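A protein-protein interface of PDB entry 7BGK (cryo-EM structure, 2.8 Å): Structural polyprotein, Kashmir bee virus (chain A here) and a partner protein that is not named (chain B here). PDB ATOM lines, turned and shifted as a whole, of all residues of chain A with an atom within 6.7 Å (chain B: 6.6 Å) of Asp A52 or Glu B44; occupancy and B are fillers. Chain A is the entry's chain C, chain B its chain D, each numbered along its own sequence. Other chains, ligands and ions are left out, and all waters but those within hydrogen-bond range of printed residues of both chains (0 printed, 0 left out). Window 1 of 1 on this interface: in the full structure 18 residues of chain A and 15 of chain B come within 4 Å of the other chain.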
ATOM      1  N   SER A  49       0.297 -17.527 -10.916  1.00  0.00           N
ATOM      2  CA  SER A  49       0.033 -18.330  -9.735  1.00  0.00           C
ATOM      3  C   SER A  49       0.755 -17.748  -8.526  1.00  0.00           C
ATOM      4  O   SER A  49       1.925 -17.356  -8.606  1.00  0.00           O
ATOM      5  CB  SER A  49       0.487 -19.755  -9.939  1.00  0.00           C
ATOM      6  OG  SER A  49       0.147 -20.566  -8.836  1.00  0.00           O
ATOM      7  N   ALA A  50       0.044 -17.696  -7.404  1.00  0.00           N
ATOM      8  CA  ALA A  50       0.584 -17.224  -6.141  1.00  0.00           C
ATOM      9  C   ALA A  50       1.339 -18.296  -5.380  1.00  0.00           C
ATOM     10  O   ALA A  50       1.653 -18.090  -4.206  1.00  0.00           O
ATOM     11  CB  ALA A  50      -0.544 -16.677  -5.273  1.00  0.00           C
ATOM     12  N   VAL A  51       1.628 -19.421  -6.002  1.00  0.00           N
ATOM     13  CA  VAL A  51       2.371 -20.498  -5.368  1.00  0.00           C
ATOM     14  C   VAL A  51       3.856 -20.281  -5.610  1.00  0.00           C
ATOM     15  O   VAL A  51       4.262 -19.794  -6.670  1.00  0.00           O
ATOM     16  CB  VAL A  51       1.909 -21.869  -5.903  1.00  0.00           C
ATOM     17  CG1 VAL A  51       2.357 -22.076  -7.323  1.00  0.00           C
ATOM     18  CG2 VAL A  51       2.428 -22.979  -5.045  1.00  0.00           C
ATOM     19  N   ASP A  52       4.668 -20.631  -4.621  1.00  0.00           N
ATOM     20  CA  ASP A  52       6.118 -20.620  -4.781  1.00  0.00           C
ATOM     21  C   ASP A  52       6.509 -21.786  -5.674  1.00  0.00           C
ATOM     22  O   ASP A  52       6.505 -22.943  -5.249  1.00  0.00           O
ATOM     23  CB  ASP A  52       6.808 -20.707  -3.427  1.00  0.00           C
ATOM     24  CG  ASP A  52       8.287 -20.447  -3.512  1.00  0.00           C
ATOM     25  OD1 ASP A  52       8.744 -19.947  -4.557  1.00  0.00           O
ATOM     26  OD2 ASP A  52       8.999 -20.736  -2.531  1.00  0.00           O
ATOM     27  N   GLU A  53       6.841 -21.482  -6.922  1.00  0.00           N
ATOM     28  CA  GLU A  53       7.203 -22.485  -7.909  1.00  0.00           C
ATOM     29  C   GLU A  53       8.696 -22.755  -7.955  1.00  0.00           C
ATOM     30  O   GLU A  53       9.134 -23.605  -8.736  1.00  0.00           O
ATOM     31  CB  GLU A  53       6.707 -22.052  -9.287  1.00  0.00           C
ATOM     32  CG  GLU A  53       5.244 -21.662  -9.306  1.00  0.00           C
ATOM     33  CD  GLU A  53       4.770 -21.198 -10.657  1.00  0.00           C
ATOM     34  OE1 GLU A  53       4.477 -22.056 -11.515  1.00  0.00           O
ATOM     35  OE2 GLU A  53       4.690 -19.969 -10.862  1.00  0.00           O
ATOM     36  N   MET A  54       9.481 -22.060  -7.140  1.00  0.00           N
ATOM     37  CA  MET A  54      10.910 -22.294  -7.032  1.00  0.00           C
ATOM     38  C   MET A  54      11.259 -23.225  -5.886  1.00  0.00           C
ATOM     39  O   MET A  54      12.442 -23.448  -5.622  1.00  0.00           O
ATOM     40  CB  MET A  54      11.648 -20.972  -6.853  1.00  0.00           C
ATOM     41  CG  MET A  54      11.398 -19.951  -7.940  1.00  0.00           C
ATOM     42  SD  MET A  54      12.270 -20.309  -9.452  1.00  0.00           S
ATOM     43  CE  MET A  54      13.912 -19.879  -8.946  1.00  0.00           C
ATOM     44  N   ALA A  55      10.263 -23.765  -5.199  1.00  0.00           N
ATOM     45  CA  ALA A  55      10.502 -24.677  -4.098  1.00  0.00           C
ATOM     46  C   ALA A  55      10.866 -26.054  -4.623  1.00  0.00           C
ATOM     47  O   ALA A  55      10.297 -26.533  -5.606  1.00  0.00           O
ATOM     48  CB  ALA A  55       9.271 -24.760  -3.206  1.00  0.00           C
ATOM     49  N   ILE A  56      11.815 -26.698  -3.946  1.00  0.00           N
ATOM     50  CA  ILE A  56      12.327 -27.978  -4.418  1.00  0.00           C
ATOM     51  C   ILE A  56      11.226 -29.025  -4.435  1.00  0.00           C
ATOM     52  O   ILE A  56      11.232 -29.929  -5.279  1.00  0.00           O
ATOM     53  CB  ILE A  56      13.531 -28.399  -3.552  1.00  0.00           C
ATOM     54  CG1 ILE A  56      14.787 -27.700  -4.066  1.00  0.00           C
ATOM     55  CG2 ILE A  56      13.719 -29.889  -3.556  1.00  0.00           C
ATOM     56  CD1 ILE A  56      16.012 -27.923  -3.245  1.00  0.00           C
ATOM     57  N   TYR A  58       8.052 -28.358  -5.124  1.00  0.00           N
ATOM     58  CA  TYR A  58       7.162 -28.059  -6.235  1.00  0.00           C
ATOM     59  C   TYR A  58       7.765 -28.487  -7.563  1.00  0.00           C
ATOM     60  O   TYR A  58       7.036 -28.915  -8.461  1.00  0.00           O
ATOM     61  CB  TYR A  58       6.841 -26.566  -6.253  1.00  0.00           C
ATOM     62  CG  TYR A  58       5.844 -26.145  -7.304  1.00  0.00           C
ATOM     63  CD1 TYR A  58       4.490 -26.182  -7.053  1.00  0.00           C
ATOM     64  CD2 TYR A  58       6.259 -25.714  -8.548  1.00  0.00           C
ATOM     65  CE1 TYR A  58       3.578 -25.799  -8.004  1.00  0.00           C
ATOM     66  CE2 TYR A  58       5.350 -25.331  -9.507  1.00  0.00           C
ATOM     67  CZ  TYR A  58       4.010 -25.377  -9.230  1.00  0.00           C
ATOM     68  OH  TYR A  58       3.092 -24.996 -10.182  1.00  0.00           O
ATOM     69  N   VAL A  59       9.085 -28.383  -7.701  1.00  0.00           N
ATOM     70  CA  VAL A  59       9.752 -28.816  -8.921  1.00  0.00           C
ATOM     71  C   VAL A  59       9.869 -30.331  -8.953  1.00  0.00           C
ATOM     72  O   VAL A  59       9.429 -30.987  -9.904  1.00  0.00           O
ATOM     73  CB  VAL A  59      11.133 -28.149  -9.043  1.00  0.00           C
ATOM     74  CG1 VAL A  59      11.715 -28.390 -10.407  1.00  0.00           C
ATOM     75  CG2 VAL A  59      11.045 -26.674  -8.774  1.00  0.00           C
ATOM     76  N   VAL B  25      13.779 -12.022   8.988  1.00  0.00           N
ATOM     77  CA  VAL B  25      12.379 -11.517   9.057  1.00  0.00           C
ATOM     78  C   VAL B  25      11.477 -12.749   9.035  1.00  0.00           C
ATOM     79  O   VAL B  25      11.718 -13.636   8.191  1.00  0.00           O
ATOM     80  CB  VAL B  25      12.061 -10.564   7.890  1.00  0.00           C
ATOM     81  CG1 VAL B  25      10.599 -10.144   7.891  1.00  0.00           C
ATOM     82  CG2 VAL B  25      12.970  -9.343   7.889  1.00  0.00           C
ATOM     83  N   ALA B  26      10.491 -12.808   9.932  1.00  0.00           N
ATOM     84  CA  ALA B  26       9.594 -13.944  10.004  1.00  0.00           C
ATOM     85  C   ALA B  26       8.665 -13.985   8.795  1.00  0.00           C
ATOM     86  O   ALA B  26       8.607 -13.067   7.973  1.00  0.00           O
ATOM     87  CB  ALA B  26       8.793 -13.899  11.299  1.00  0.00           C
ATOM     88  N   SER B  27       7.927 -15.093   8.702  1.00  0.00           N
ATOM     89  CA  SER B  27       7.155 -15.420   7.505  1.00  0.00           C
ATOM     90  C   SER B  27       5.656 -15.546   7.753  1.00  0.00           C
ATOM     91  O   SER B  27       4.896 -14.749   7.198  1.00  0.00           O
ATOM     92  CB  SER B  27       7.734 -16.675   6.862  1.00  0.00           C
ATOM     93  OG  SER B  27       7.514 -17.846   7.617  1.00  0.00           O
ATOM     94  N   GLY B  28       5.189 -16.505   8.557  1.00  0.00           N
ATOM     95  CA  GLY B  28       3.767 -16.801   8.572  1.00  0.00           C
ATOM     96  C   GLY B  28       3.341 -17.820   7.536  1.00  0.00           C
ATOM     97  O   GLY B  28       2.217 -17.754   7.021  1.00  0.00           O
ATOM     98  N   VAL B  29       4.245 -18.763   7.223  1.00  0.00           N
ATOM     99  CA  VAL B  29       3.871 -19.912   6.343  1.00  0.00           C
ATOM    100  C   VAL B  29       3.787 -21.125   7.277  1.00  0.00           C
ATOM    101  O   VAL B  29       4.387 -21.050   8.368  1.00  0.00           O
ATOM    102  CB  VAL B  29       4.851 -20.170   5.180  1.00  0.00           C
ATOM    103  CG1 VAL B  29       4.484 -21.423   4.397  1.00  0.00           C
ATOM    104  CG2 VAL B  29       4.976 -18.985   4.247  1.00  0.00           C
ATOM    105  N   ARG B  38       1.618 -27.495  -1.949  1.00  0.00           N
ATOM    106  CA  ARG B  38       1.715 -26.178  -2.561  1.00  0.00           C
ATOM    107  C   ARG B  38       1.656 -25.094  -1.494  1.00  0.00           C
ATOM    108  O   ARG B  38       0.732 -25.064  -0.678  1.00  0.00           O
ATOM    109  CB  ARG B  38       0.600 -25.993  -3.588  1.00  0.00           C
ATOM    110  CG  ARG B  38       0.574 -27.061  -4.682  1.00  0.00           C
ATOM    111  CD  ARG B  38       1.850 -26.995  -5.521  1.00  0.00           C
ATOM    112  NE  ARG B  38       1.899 -27.901  -6.676  1.00  0.00           N
ATOM    113  CZ  ARG B  38       2.564 -29.055  -6.719  1.00  0.00           C
ATOM    114  NH1 ARG B  38       2.561 -29.781  -7.829  1.00  0.00           N
ATOM    115  NH2 ARG B  38       3.240 -29.495  -5.673  1.00  0.00           N
ATOM    116  N   ILE B  39       2.646 -24.207  -1.499  1.00  0.00           N
ATOM    117  CA  ILE B  39       2.756 -23.175  -0.473  1.00  0.00           C
ATOM    118  C   ILE B  39       2.687 -21.797  -1.120  1.00  0.00           C
ATOM    119  O   ILE B  39       3.272 -21.592  -2.191  1.00  0.00           O
ATOM    120  CB  ILE B  39       4.056 -23.332   0.325  1.00  0.00           C
ATOM    121  CG1 ILE B  39       5.273 -23.160  -0.564  1.00  0.00           C
ATOM    122  CG2 ILE B  39       4.098 -24.702   0.933  1.00  0.00           C
ATOM    123  CD1 ILE B  39       6.568 -23.175   0.196  1.00  0.00           C
ATOM    124  N   PRO B  40       2.000 -20.826  -0.521  1.00  0.00           N
ATOM    125  CA  PRO B  40       1.907 -19.511  -1.154  1.00  0.00           C
ATOM    126  C   PRO B  40       3.219 -18.758  -1.061  1.00  0.00           C
ATOM    127  O   PRO B  40       3.993 -18.916  -0.116  1.00  0.00           O
ATOM    128  CB  PRO B  40       0.808 -18.806  -0.354  1.00  0.00           C
ATOM    129  CG  PRO B  40       0.149 -19.859   0.431  1.00  0.00           C
ATOM    130  CD  PRO B  40       1.174 -20.884   0.693  1.00  0.00           C
ATOM    131  N   VAL B  41       3.455 -17.914  -2.059  1.00  0.00           N
ATOM    132  CA  VAL B  41       4.656 -17.094  -2.077  1.00  0.00           C
ATOM    133  C   VAL B  41       4.471 -15.767  -1.351  1.00  0.00           C
ATOM    134  O   VAL B  41       5.466 -15.110  -1.017  1.00  0.00           O
ATOM    135  CB  VAL B  41       5.104 -16.871  -3.532  1.00  0.00           C
ATOM    136  CG1 VAL B  41       4.193 -15.892  -4.247  1.00  0.00           C
ATOM    137  CG2 VAL B  41       6.533 -16.421  -3.582  1.00  0.00           C
ATOM    138  N   LEU B  42       3.231 -15.356  -1.096  1.00  0.00           N
ATOM    139  CA  LEU B  42       2.990 -14.100  -0.409  1.00  0.00           C
ATOM    140  C   LEU B  42       3.187 -14.209   1.092  1.00  0.00           C
ATOM    141  O   LEU B  42       3.421 -13.192   1.752  1.00  0.00           O
ATOM    142  CB  LEU B  42       1.572 -13.628  -0.703  1.00  0.00           C
ATOM    143  CG  LEU B  42       1.304 -13.177  -2.135  1.00  0.00           C
ATOM    144  CD1 LEU B  42      -0.160 -12.894  -2.333  1.00  0.00           C
ATOM    145  CD2 LEU B  42       2.118 -11.964  -2.456  1.00  0.00           C
ATOM    146  N   GLY B  43       3.077 -15.416   1.643  1.00  0.00           N
ATOM    147  CA  GLY B  43       3.390 -15.655   3.035  1.00  0.00           C
ATOM    148  C   GLY B  43       4.863 -15.787   3.335  1.00  0.00           C
ATOM    149  O   GLY B  43       5.271 -15.593   4.483  1.00  0.00           O
ATOM    150  N   GLU B  44       5.670 -16.111   2.327  1.00  0.00           N
ATOM    151  CA  GLU B  44       7.095 -16.314   2.545  1.00  0.00           C
ATOM    152  C   GLU B  44       7.867 -15.017   2.732  1.00  0.00           C
ATOM    153  O   GLU B  44       8.719 -14.928   3.623  1.00  0.00           O
ATOM    154  CB  GLU B  44       7.678 -17.057   1.347  1.00  0.00           C
ATOM    155  CG  GLU B  44       7.082 -18.411   1.079  1.00  0.00           C
ATOM    156  CD  GLU B  44       7.598 -19.012  -0.204  1.00  0.00           C
ATOM    157  OE1 GLU B  44       8.367 -18.329  -0.909  1.00  0.00           O
ATOM    158  OE2 GLU B  44       7.238 -20.166  -0.508  1.00  0.00           O
ATOM    159  N   ILE B  45       7.587 -14.004   1.925  1.00  0.00           N
ATOM    160  CA  ILE B  45       7.824 -12.612   2.275  1.00  0.00           C
ATOM    161  C   ILE B  45       6.517 -11.843   2.215  1.00  0.00           C
ATOM    162  O   ILE B  45       5.700 -12.062   1.315  1.00  0.00           O
ATOM    163  CB  ILE B  45       8.871 -11.975   1.337  1.00  0.00           C
ATOM    164  CG1 ILE B  45       9.290 -10.591   1.826  1.00  0.00           C
ATOM    165  CG2 ILE B  45       8.324 -11.861  -0.075  1.00  0.00           C
ATOM    166  CD1 ILE B  45       9.780 -10.532   3.243  1.00  0.00           C
ATOM    167  N   ALA B  46       6.322 -10.937   3.164  1.00  0.00           N
ATOM    168  CA  ALA B  46       5.179 -10.037   3.136  1.00  0.00           C
ATOM    169  C   ALA B  46       5.716  -8.638   2.867  1.00  0.00           C
ATOM    170  O   ALA B  46       6.403  -8.054   3.712  1.00  0.00           O
ATOM    171  CB  ALA B  46       4.407 -10.085   4.450  1.00  0.00           C
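O of Ile B39 is in hydrogen-bond range of N of Asp A52. N of Val B41 lies within hydrogen-bond range of O of Ala A50, at 2.8 Å. OE2 of Glu B44 lies close to OD2 of Asp A52, 2.7 Å away.
OG of Ser A49 sits close to N of Val A51, at 3.4 Å. The side-chain carboxylate of Asp A52 lies close to the backbone NH of Met A54 (3.4 Å).
Ala A50 touches Pro B40 (O to CA, 3.4 Å). CB of Arg B38 touches CG2 of Val A51, at 3.8 Å. Ile B39 touches Val A51 (O to CG2, 3.3 Å). Asp A52 touches Val B41. Tyr A58 touches Arg B38.
Of chain B, only Ile B39 (3.0 Å), Val B41 (3.9 Å) and Glu B44 (2.7 Å) come within 4 Å of Asp A52. Glu B44 touches just one residue of chain A: Asp A52. Of the printed residues of chain B, Ala A50 touches Pro B40 and Val B41. Of the printed residues of chain A, Val B41 touches Ala A50 (2.8 Å) and Asp A52 (3.9 Å). Printed residues of chain B within 4 Å of Val A51: Arg B38 (3.8 Å) and Ile B39 (3.3 Å). Of the printed residues of chain A, Ile B39 touches Val A51 and Asp A52. Of the printed residues of chain A, Arg B38 touches Val A51 and Tyr A58. The nearest residue of chain B that does not touch Asp A52 is Pro B40 (4.3 Å).
Printed residues of chain A that touch a printed residue of chain B: Ala A50, Val A51, Asp A52 and Tyr A58. Hydrophobic or aromatic side chains of chain A within 4 Å of the printed part of chain B: Val A51 and Tyr A58. Hydrophobic or aromatic side chains of chain B that line the printed part of chain A: Val B41. Among the printed residues, 8 pairs touch across the chains.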
